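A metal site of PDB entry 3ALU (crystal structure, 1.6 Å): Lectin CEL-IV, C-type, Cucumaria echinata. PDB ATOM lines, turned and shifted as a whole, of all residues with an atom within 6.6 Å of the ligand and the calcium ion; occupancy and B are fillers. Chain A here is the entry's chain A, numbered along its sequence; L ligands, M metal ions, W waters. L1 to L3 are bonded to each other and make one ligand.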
ATOM      1  N   GLY A  77      26.860 -12.361  -9.241  1.00  0.00           N
ATOM      2  CA  GLY A  77      27.704 -12.868 -10.330  1.00  0.00           C
ATOM      3  C   GLY A  77      27.443 -14.332 -10.599  1.00  0.00           C
ATOM      4  O   GLY A  77      27.980 -14.878 -11.565  1.00  0.00           O
ATOM      5  N   GLY A  78      26.664 -14.976  -9.718  1.00  0.00           N
ATOM      6  CA  GLY A  78      26.347 -16.411  -9.851  1.00  0.00           C
ATOM      7  C   GLY A  78      25.008 -16.646 -10.558  1.00  0.00           C
ATOM      8  O   GLY A  78      24.646 -15.878 -11.435  1.00  0.00           O
ATOM      9  N   TRP A  79      24.321 -17.715 -10.190  1.00  0.00           N
ATOM     10  CA  TRP A  79      22.969 -17.988 -10.657  1.00  0.00           C
ATOM     11  C   TRP A  79      21.927 -17.112  -9.982  1.00  0.00           C
ATOM     12  O   TRP A  79      20.879 -16.816 -10.594  1.00  0.00           O
ATOM     13  CB  TRP A  79      22.612 -19.454 -10.348  1.00  0.00           C
ATOM     14  CG  TRP A  79      23.581 -20.456 -10.944  1.00  0.00           C
ATOM     15  CD1 TRP A  79      24.760 -20.896 -10.382  1.00  0.00           C
ATOM     16  CD2 TRP A  79      23.429 -21.182 -12.184  1.00  0.00           C
ATOM     17  NE1 TRP A  79      25.346 -21.831 -11.208  1.00  0.00           N
ATOM     18  CE2 TRP A  79      24.565 -22.020 -12.313  1.00  0.00           C
ATOM     19  CE3 TRP A  79      22.467 -21.177 -13.212  1.00  0.00           C
ATOM     20  CZ2 TRP A  79      24.745 -22.871 -13.410  1.00  0.00           C
ATOM     21  CZ3 TRP A  79      22.636 -22.020 -14.295  1.00  0.00           C
ATOM     22  CH2 TRP A  79      23.793 -22.849 -14.399  1.00  0.00           C
ATOM     23  N   ALA A  80      22.181 -16.760  -8.727  1.00  0.00           N
ATOM     24  CA  ALA A  80      21.204 -16.077  -7.867  1.00  0.00           C
ATOM     25  C   ALA A  80      20.930 -14.672  -8.364  1.00  0.00           C
ATOM     26  O   ALA A  80      21.853 -13.972  -8.770  1.00  0.00           O
ATOM     27  CB  ALA A  80      21.710 -16.015  -6.390  1.00  0.00           C
ATOM     28  N   GLN A  82      17.438 -17.122  -8.077  1.00  0.00           N
ATOM     29  CA  GLN A  82      16.732 -18.133  -8.837  1.00  0.00           C
ATOM     30  C   GLN A  82      15.267 -18.032  -8.464  1.00  0.00           C
ATOM     31  O   GLN A  82      14.936 -17.935  -7.297  1.00  0.00           O
ATOM     32  CB  GLN A  82      17.282 -19.499  -8.473  1.00  0.00           C
ATOM     33  CG  GLN A  82      18.728 -19.570  -8.837  1.00  0.00           C
ATOM     34  CD  GLN A  82      19.330 -20.936  -8.532  1.00  0.00           C
ATOM     35  OE1 GLN A  82      19.989 -21.118  -7.504  1.00  0.00           O
ATOM     36  NE2 GLN A  82      19.092 -21.894  -9.410  1.00  0.00           N
ATOM     37  N   GLY A 112      24.337 -26.952 -20.464  1.00  0.00           N
ATOM     38  CA  GLY A 112      24.598 -27.950 -19.422  1.00  0.00           C
ATOM     39  C   GLY A 112      23.461 -28.302 -18.467  1.00  0.00           C
ATOM     40  O   GLY A 112      23.600 -29.225 -17.625  1.00  0.00           O
ATOM     41  N   GLU A 113      22.363 -27.536 -18.547  1.00  0.00           N
ATOM     42  CA  GLU A 113      21.102 -27.827 -17.826  1.00  0.00           C
ATOM     43  C   GLU A 113      20.063 -28.418 -18.769  1.00  0.00           C
ATOM     44  O   GLU A 113      20.032 -28.095 -19.959  1.00  0.00           O
ATOM     45  CB  GLU A 113      20.532 -26.551 -17.201  1.00  0.00           C
ATOM     46  CG  GLU A 113      21.517 -25.701 -16.405  1.00  0.00           C
ATOM     47  CD  GLU A 113      21.932 -26.323 -15.081  1.00  0.00           C
ATOM     48  OE1 GLU A 113      23.154 -26.450 -14.849  1.00  0.00           O
ATOM     49  OE2 GLU A 113      21.057 -26.644 -14.251  1.00  0.00           O
ATOM     50  N   PRO A 114      19.187 -29.312 -18.263  1.00  0.00           N
ATOM     51  CA  PRO A 114      19.110 -29.823 -16.885  1.00  0.00           C
ATOM     52  C   PRO A 114      20.177 -30.865 -16.615  1.00  0.00           C
ATOM     53  O   PRO A 114      20.519 -31.649 -17.514  1.00  0.00           O
ATOM     54  CB  PRO A 114      17.706 -30.489 -16.822  1.00  0.00           C
ATOM     55  CG  PRO A 114      17.367 -30.806 -18.236  1.00  0.00           C
ATOM     56  CD  PRO A 114      18.104 -29.822 -19.121  1.00  0.00           C
ATOM     57  N   ASN A 115      20.700 -30.872 -15.406  1.00  0.00           N
ATOM     58  CA  ASN A 115      21.759 -31.829 -15.053  1.00  0.00           C
ATOM     59  C   ASN A 115      21.563 -32.444 -13.675  1.00  0.00           C
ATOM     60  O   ASN A 115      22.448 -33.156 -13.159  1.00  0.00           O
ATOM     61  CB  ASN A 115      23.112 -31.123 -15.153  1.00  0.00           C
ATOM     62  CG  ASN A 115      23.264 -30.007 -14.129  1.00  0.00           C
ATOM     63  OD1 ASN A 115      22.282 -29.500 -13.560  1.00  0.00           O
ATOM     64  ND2 ASN A 115      24.501 -29.623 -13.865  1.00  0.00           N
ATOM     65  N   ASN A 116      20.394 -32.185 -13.070  1.00  0.00           N
ATOM     66  CA  ASN A 116      20.089 -32.679 -11.713  1.00  0.00           C
ATOM     67  C   ASN A 116      18.929 -33.662 -11.685  1.00  0.00           C
ATOM     68  O   ASN A 116      18.391 -33.971 -10.611  1.00  0.00           O
ATOM     69  CB  ASN A 116      19.881 -31.528 -10.710  1.00  0.00           C
ATOM     70  CG  ASN A 116      21.163 -30.784 -10.422  1.00  0.00           C
ATOM     71  OD1 ASN A 116      21.301 -29.608 -10.764  1.00  0.00           O
ATOM     72  ND2 ASN A 116      22.147 -31.484  -9.822  1.00  0.00           N
ATOM     73  N   SER A 120      13.839 -33.143 -11.078  1.00  0.00           N
ATOM     74  CA  SER A 120      14.318 -31.791 -10.696  1.00  0.00           C
ATOM     75  C   SER A 120      13.302 -30.756 -11.190  1.00  0.00           C
ATOM     76  O   SER A 120      12.364 -31.107 -11.907  1.00  0.00           O
ATOM     77  CB  SER A 120      15.684 -31.503 -11.304  1.00  0.00           C
ATOM     78  OG  SER A 120      15.656 -31.759 -12.724  1.00  0.00           O
ATOM     79  N   ALA A 125      17.266 -18.311 -13.633  1.00  0.00           N
ATOM     80  CA  ALA A 125      18.428 -17.995 -12.818  1.00  0.00           C
ATOM     81  C   ALA A 125      18.882 -16.617 -13.265  1.00  0.00           C
ATOM     82  O   ALA A 125      19.567 -16.476 -14.273  1.00  0.00           O
ATOM     83  CB  ALA A 125      19.516 -19.079 -13.001  1.00  0.00           C
ATOM     84  N   TYR A 129      25.668 -15.109 -14.102  1.00  0.00           N
ATOM     85  CA  TYR A 129      26.240 -16.323 -14.693  1.00  0.00           C
ATOM     86  C   TYR A 129      25.325 -16.856 -15.802  1.00  0.00           C
ATOM     87  O   TYR A 129      25.774 -17.380 -16.808  1.00  0.00           O
ATOM     88  CB  TYR A 129      26.450 -17.400 -13.615  1.00  0.00           C
ATOM     89  CG  TYR A 129      27.112 -18.644 -14.161  1.00  0.00           C
ATOM     90  CD1 TYR A 129      28.435 -18.579 -14.606  1.00  0.00           C
ATOM     91  CD2 TYR A 129      26.426 -19.836 -14.253  1.00  0.00           C
ATOM     92  CE1 TYR A 129      29.055 -19.683 -15.158  1.00  0.00           C
ATOM     93  CE2 TYR A 129      27.054 -20.985 -14.799  1.00  0.00           C
ATOM     94  CZ  TYR A 129      28.370 -20.879 -15.220  1.00  0.00           C
ATOM     95  OH  TYR A 129      29.017 -21.954 -15.755  1.00  0.00           O
ATOM     96  N   ALA A 135      17.966 -22.933 -14.774  1.00  0.00           N
ATOM     97  CA  ALA A 135      18.725 -23.994 -14.097  1.00  0.00           C
ATOM     98  C   ALA A 135      17.737 -25.011 -13.586  1.00  0.00           C
ATOM     99  O   ALA A 135      16.601 -24.645 -13.234  1.00  0.00           O
ATOM    100  CB  ALA A 135      19.532 -23.427 -12.923  1.00  0.00           C
ATOM    101  N   ASP A 136      18.112 -26.288 -13.528  1.00  0.00           N
ATOM    102  CA  ASP A 136      17.271 -27.212 -12.763  1.00  0.00           C
ATOM    103  C   ASP A 136      17.851 -27.415 -11.373  1.00  0.00           C
ATOM    104  O   ASP A 136      19.085 -27.331 -11.178  1.00  0.00           O
ATOM    105  CB  ASP A 136      17.003 -28.558 -13.465  1.00  0.00           C
ATOM    106  CG  ASP A 136      18.230 -29.501 -13.499  1.00  0.00           C
ATOM    107  OD1 ASP A 136      19.369 -29.036 -13.617  1.00  0.00           O
ATOM    108  OD2 ASP A 136      18.025 -30.725 -13.449  1.00  0.00           O
ATOM    109  N   VAL A 137      16.936 -27.577 -10.419  1.00  0.00           N
ATOM    110  CA  VAL A 137      17.306 -27.644  -9.009  1.00  0.00           C
ATOM    111  C   VAL A 137      16.478 -28.705  -8.332  1.00  0.00           C
ATOM    112  O   VAL A 137      15.430 -29.112  -8.816  1.00  0.00           O
ATOM    113  CB  VAL A 137      17.052 -26.274  -8.279  1.00  0.00           C
ATOM    114  CG1 VAL A 137      17.861 -25.108  -8.895  1.00  0.00           C
ATOM    115  CG2 VAL A 137      15.546 -25.935  -8.186  1.00  0.00           C
ATOM    116  N   ASN A 141      14.489 -26.816  -2.645  1.00  0.00           N
ATOM    117  CA  ASN A 141      14.967 -25.432  -2.594  1.00  0.00           C
ATOM    118  C   ASN A 141      13.819 -24.453  -2.407  1.00  0.00           C
ATOM    119  O   ASN A 141      12.806 -24.584  -3.065  1.00  0.00           O
ATOM    120  CB  ASN A 141      15.719 -25.076  -3.883  1.00  0.00           C
ATOM    121  CG  ASN A 141      17.137 -25.569  -3.864  1.00  0.00           C
ATOM    122  OD1 ASN A 141      17.464 -26.606  -4.476  1.00  0.00           O
ATOM    123  ND2 ASN A 141      17.992 -24.878  -3.142  1.00  0.00           N
ATOM    124  N   PHE A 143      12.610 -20.881  -3.023  1.00  0.00           N
ATOM    125  CA  PHE A 143      12.875 -19.718  -3.866  1.00  0.00           C
ATOM    126  C   PHE A 143      11.635 -18.812  -4.017  1.00  0.00           C
ATOM    127  O   PHE A 143      10.492 -19.225  -3.793  1.00  0.00           O
ATOM    128  CB  PHE A 143      13.214 -20.154  -5.311  1.00  0.00           C
ATOM    129  CG  PHE A 143      14.503 -20.911  -5.511  1.00  0.00           C
ATOM    130  CD1 PHE A 143      14.595 -21.777  -6.613  1.00  0.00           C
ATOM    131  CD2 PHE A 143      15.626 -20.746  -4.689  1.00  0.00           C
ATOM    132  CE1 PHE A 143      15.779 -22.453  -6.904  1.00  0.00           C
ATOM    133  CE2 PHE A 143      16.817 -21.470  -4.945  1.00  0.00           C
ATOM    134  CZ  PHE A 143      16.873 -22.339  -6.044  1.00  0.00           C
HETATM  135  C1  LIG L   1      31.316 -22.169 -12.666  1.00  0.00           C
HETATM  136  C2  LIG L   1      30.533 -23.352 -12.062  1.00  0.00           C
HETATM  137  C3  LIG L   1      31.347 -24.650 -12.114  1.00  0.00           C
HETATM  138  C4  LIG L   1      30.263 -25.725 -12.125  1.00  0.00           C
HETATM  139  C5  LIG L   1      29.067 -25.064 -12.825  1.00  0.00           C
HETATM  140  C6  LIG L   1      27.784 -25.362 -12.075  1.00  0.00           C
HETATM  141  O1  LIG L   1      31.625 -22.434 -14.043  1.00  0.00           O
HETATM  142  O2  LIG L   1      30.149 -23.060 -10.704  1.00  0.00           O
HETATM  143  O3  LIG L   1      32.242 -24.794 -11.009  1.00  0.00           O
HETATM  144  O4  LIG L   1      30.672 -26.921 -12.799  1.00  0.00           O
HETATM  145  O5  LIG L   1      29.332 -23.636 -12.828  1.00  0.00           O
HETATM  146  O6  LIG L   1      27.113 -26.455 -12.699  1.00  0.00           O
HETATM  147  C1  LG2 L   2      28.957 -22.234 -10.598  1.00  0.00           C
HETATM  148  C2  LG2 L   2      29.233 -21.050  -9.675  1.00  0.00           C
HETATM  149  C3  LG2 L   2      29.318 -21.514  -8.228  1.00  0.00           C
HETATM  150  C4  LG2 L   2      28.067 -22.284  -7.824  1.00  0.00           C
HETATM  151  C5  LG2 L   2      27.724 -23.410  -8.792  1.00  0.00           C
HETATM  152  C6  LG2 L   2      26.373 -24.039  -8.399  1.00  0.00           C
HETATM  153  O1  LG2 L   2      30.474 -20.447 -10.067  1.00  0.00           O
HETATM  154  O2  LG2 L   2      29.475 -20.363  -7.378  1.00  0.00           O
HETATM  155  O3  LG2 L   2      28.303 -22.854  -6.532  1.00  0.00           O
HETATM  156  O4  LG2 L   2      27.793 -22.960 -10.167  1.00  0.00           O
HETATM  157  O5  LG2 L   2      25.810 -24.884  -9.419  1.00  0.00           O
HETATM  158  C1  LG3 L   3      24.629 -25.628  -9.061  1.00  0.00           C
HETATM  159  C2  LG3 L   3      24.353 -26.693 -10.129  1.00  0.00           C
HETATM  160  C3  LG3 L   3      23.921 -26.104 -11.460  1.00  0.00           C
HETATM  161  C4  LG3 L   3      22.735 -25.145 -11.276  1.00  0.00           C
HETATM  162  C5  LG3 L   3      23.064 -24.136 -10.159  1.00  0.00           C
HETATM  163  C6  LG3 L   3      21.903 -23.194  -9.832  1.00  0.00           C
HETATM  164  O1  LG3 L   3      25.556 -27.467 -10.386  1.00  0.00           O
HETATM  165  O2  LG3 L   3      23.588 -27.167 -12.361  1.00  0.00           O
HETATM  166  O3  LG3 L   3      21.608 -25.942 -10.898  1.00  0.00           O
HETATM  167  O4  LG3 L   3      23.425 -24.817  -8.940  1.00  0.00           O
HETATM  168  O5  LG3 L   3      20.834 -23.977  -9.291  1.00  0.00           O
HETATM  169 CA    CA M   1      21.123 -27.969 -12.324  1.00  0.00          CA
HETATM  170  O   HOH W   1      27.481 -24.343 -15.640  1.00  0.00           O
HETATM  171  O   HOH W   2      24.857 -30.226  -9.398  1.00  0.00           O
HETATM  172  O   HOH W   3      30.370 -17.602  -9.049  1.00  0.00           O
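The side-chain hydroxyl (OH) of Tyr 129 lies within hydrogen-bond range of an oxygen (O1) of LIG L1 (3.2 Å).
The indole nitrogen (NE1) of Trp 79 sits at hydrogen-bond distance from an oxygen (O4) of LG2 L2, 2.9 Å away.
An oxygen (O5) of LG3 L3 lies within hydrogen-bond range of the side-chain amide nitrogen (NE2) of Gln 82 (2.7 Å).
The backbone carbonyl oxygen (O) of Gly 77 is in hydrogen-bond range of the backbone NH (N) of Tyr 129, 3.4 Å away.
The side-chain hydroxyl of Ser 120 lies within hydrogen-bond range of the side-chain carboxylate of Asp 136 (2.7 Å).
O of Gly 78 is in hydrogen-bond range of N of Tyr 129 (3.0 Å).
CB of Ala 135 touches O3 of LG3 L3, at 3.8 Å.
CG1 of Val 137 touches O5 of LG3 L3, 3.2 Å away.
Hydrophobic or aromatic side chains within 4 Å of the ligand: Trp 79, Tyr 129, Ala 135 and Val 137.
Of the 18 residues printed, 9 come within 4 Å of the ligand.
Within 4 Å of the calcium ion: Glu 113, Asn 115, Asn 116 and Asp 136.
The calcium ion is bound by OD1 of Asn 116 (2.3 Å), OD1 of Asn 115 (2.3 Å), OE2 of Glu 113 (2.3 Å), O of Asp 136 (2.4 Å), OD1 of Asp 136 (2.4 Å), O3 of LG3 L3 (2.5 Å) and O2 of LG3 L3 (2.6 Å).
Water W2 lies within hydrogen-bond range of an oxygen (O1) of LG3 L3 (3.0 Å) and the side-chain amide nitrogen of Asn 116 (3.0 Å).
Water W1 lies within hydrogen-bond range of the side-chain hydroxyl of Tyr 129 (2.8 Å) and an oxygen (O5) of LIG L1 (3.4 Å).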
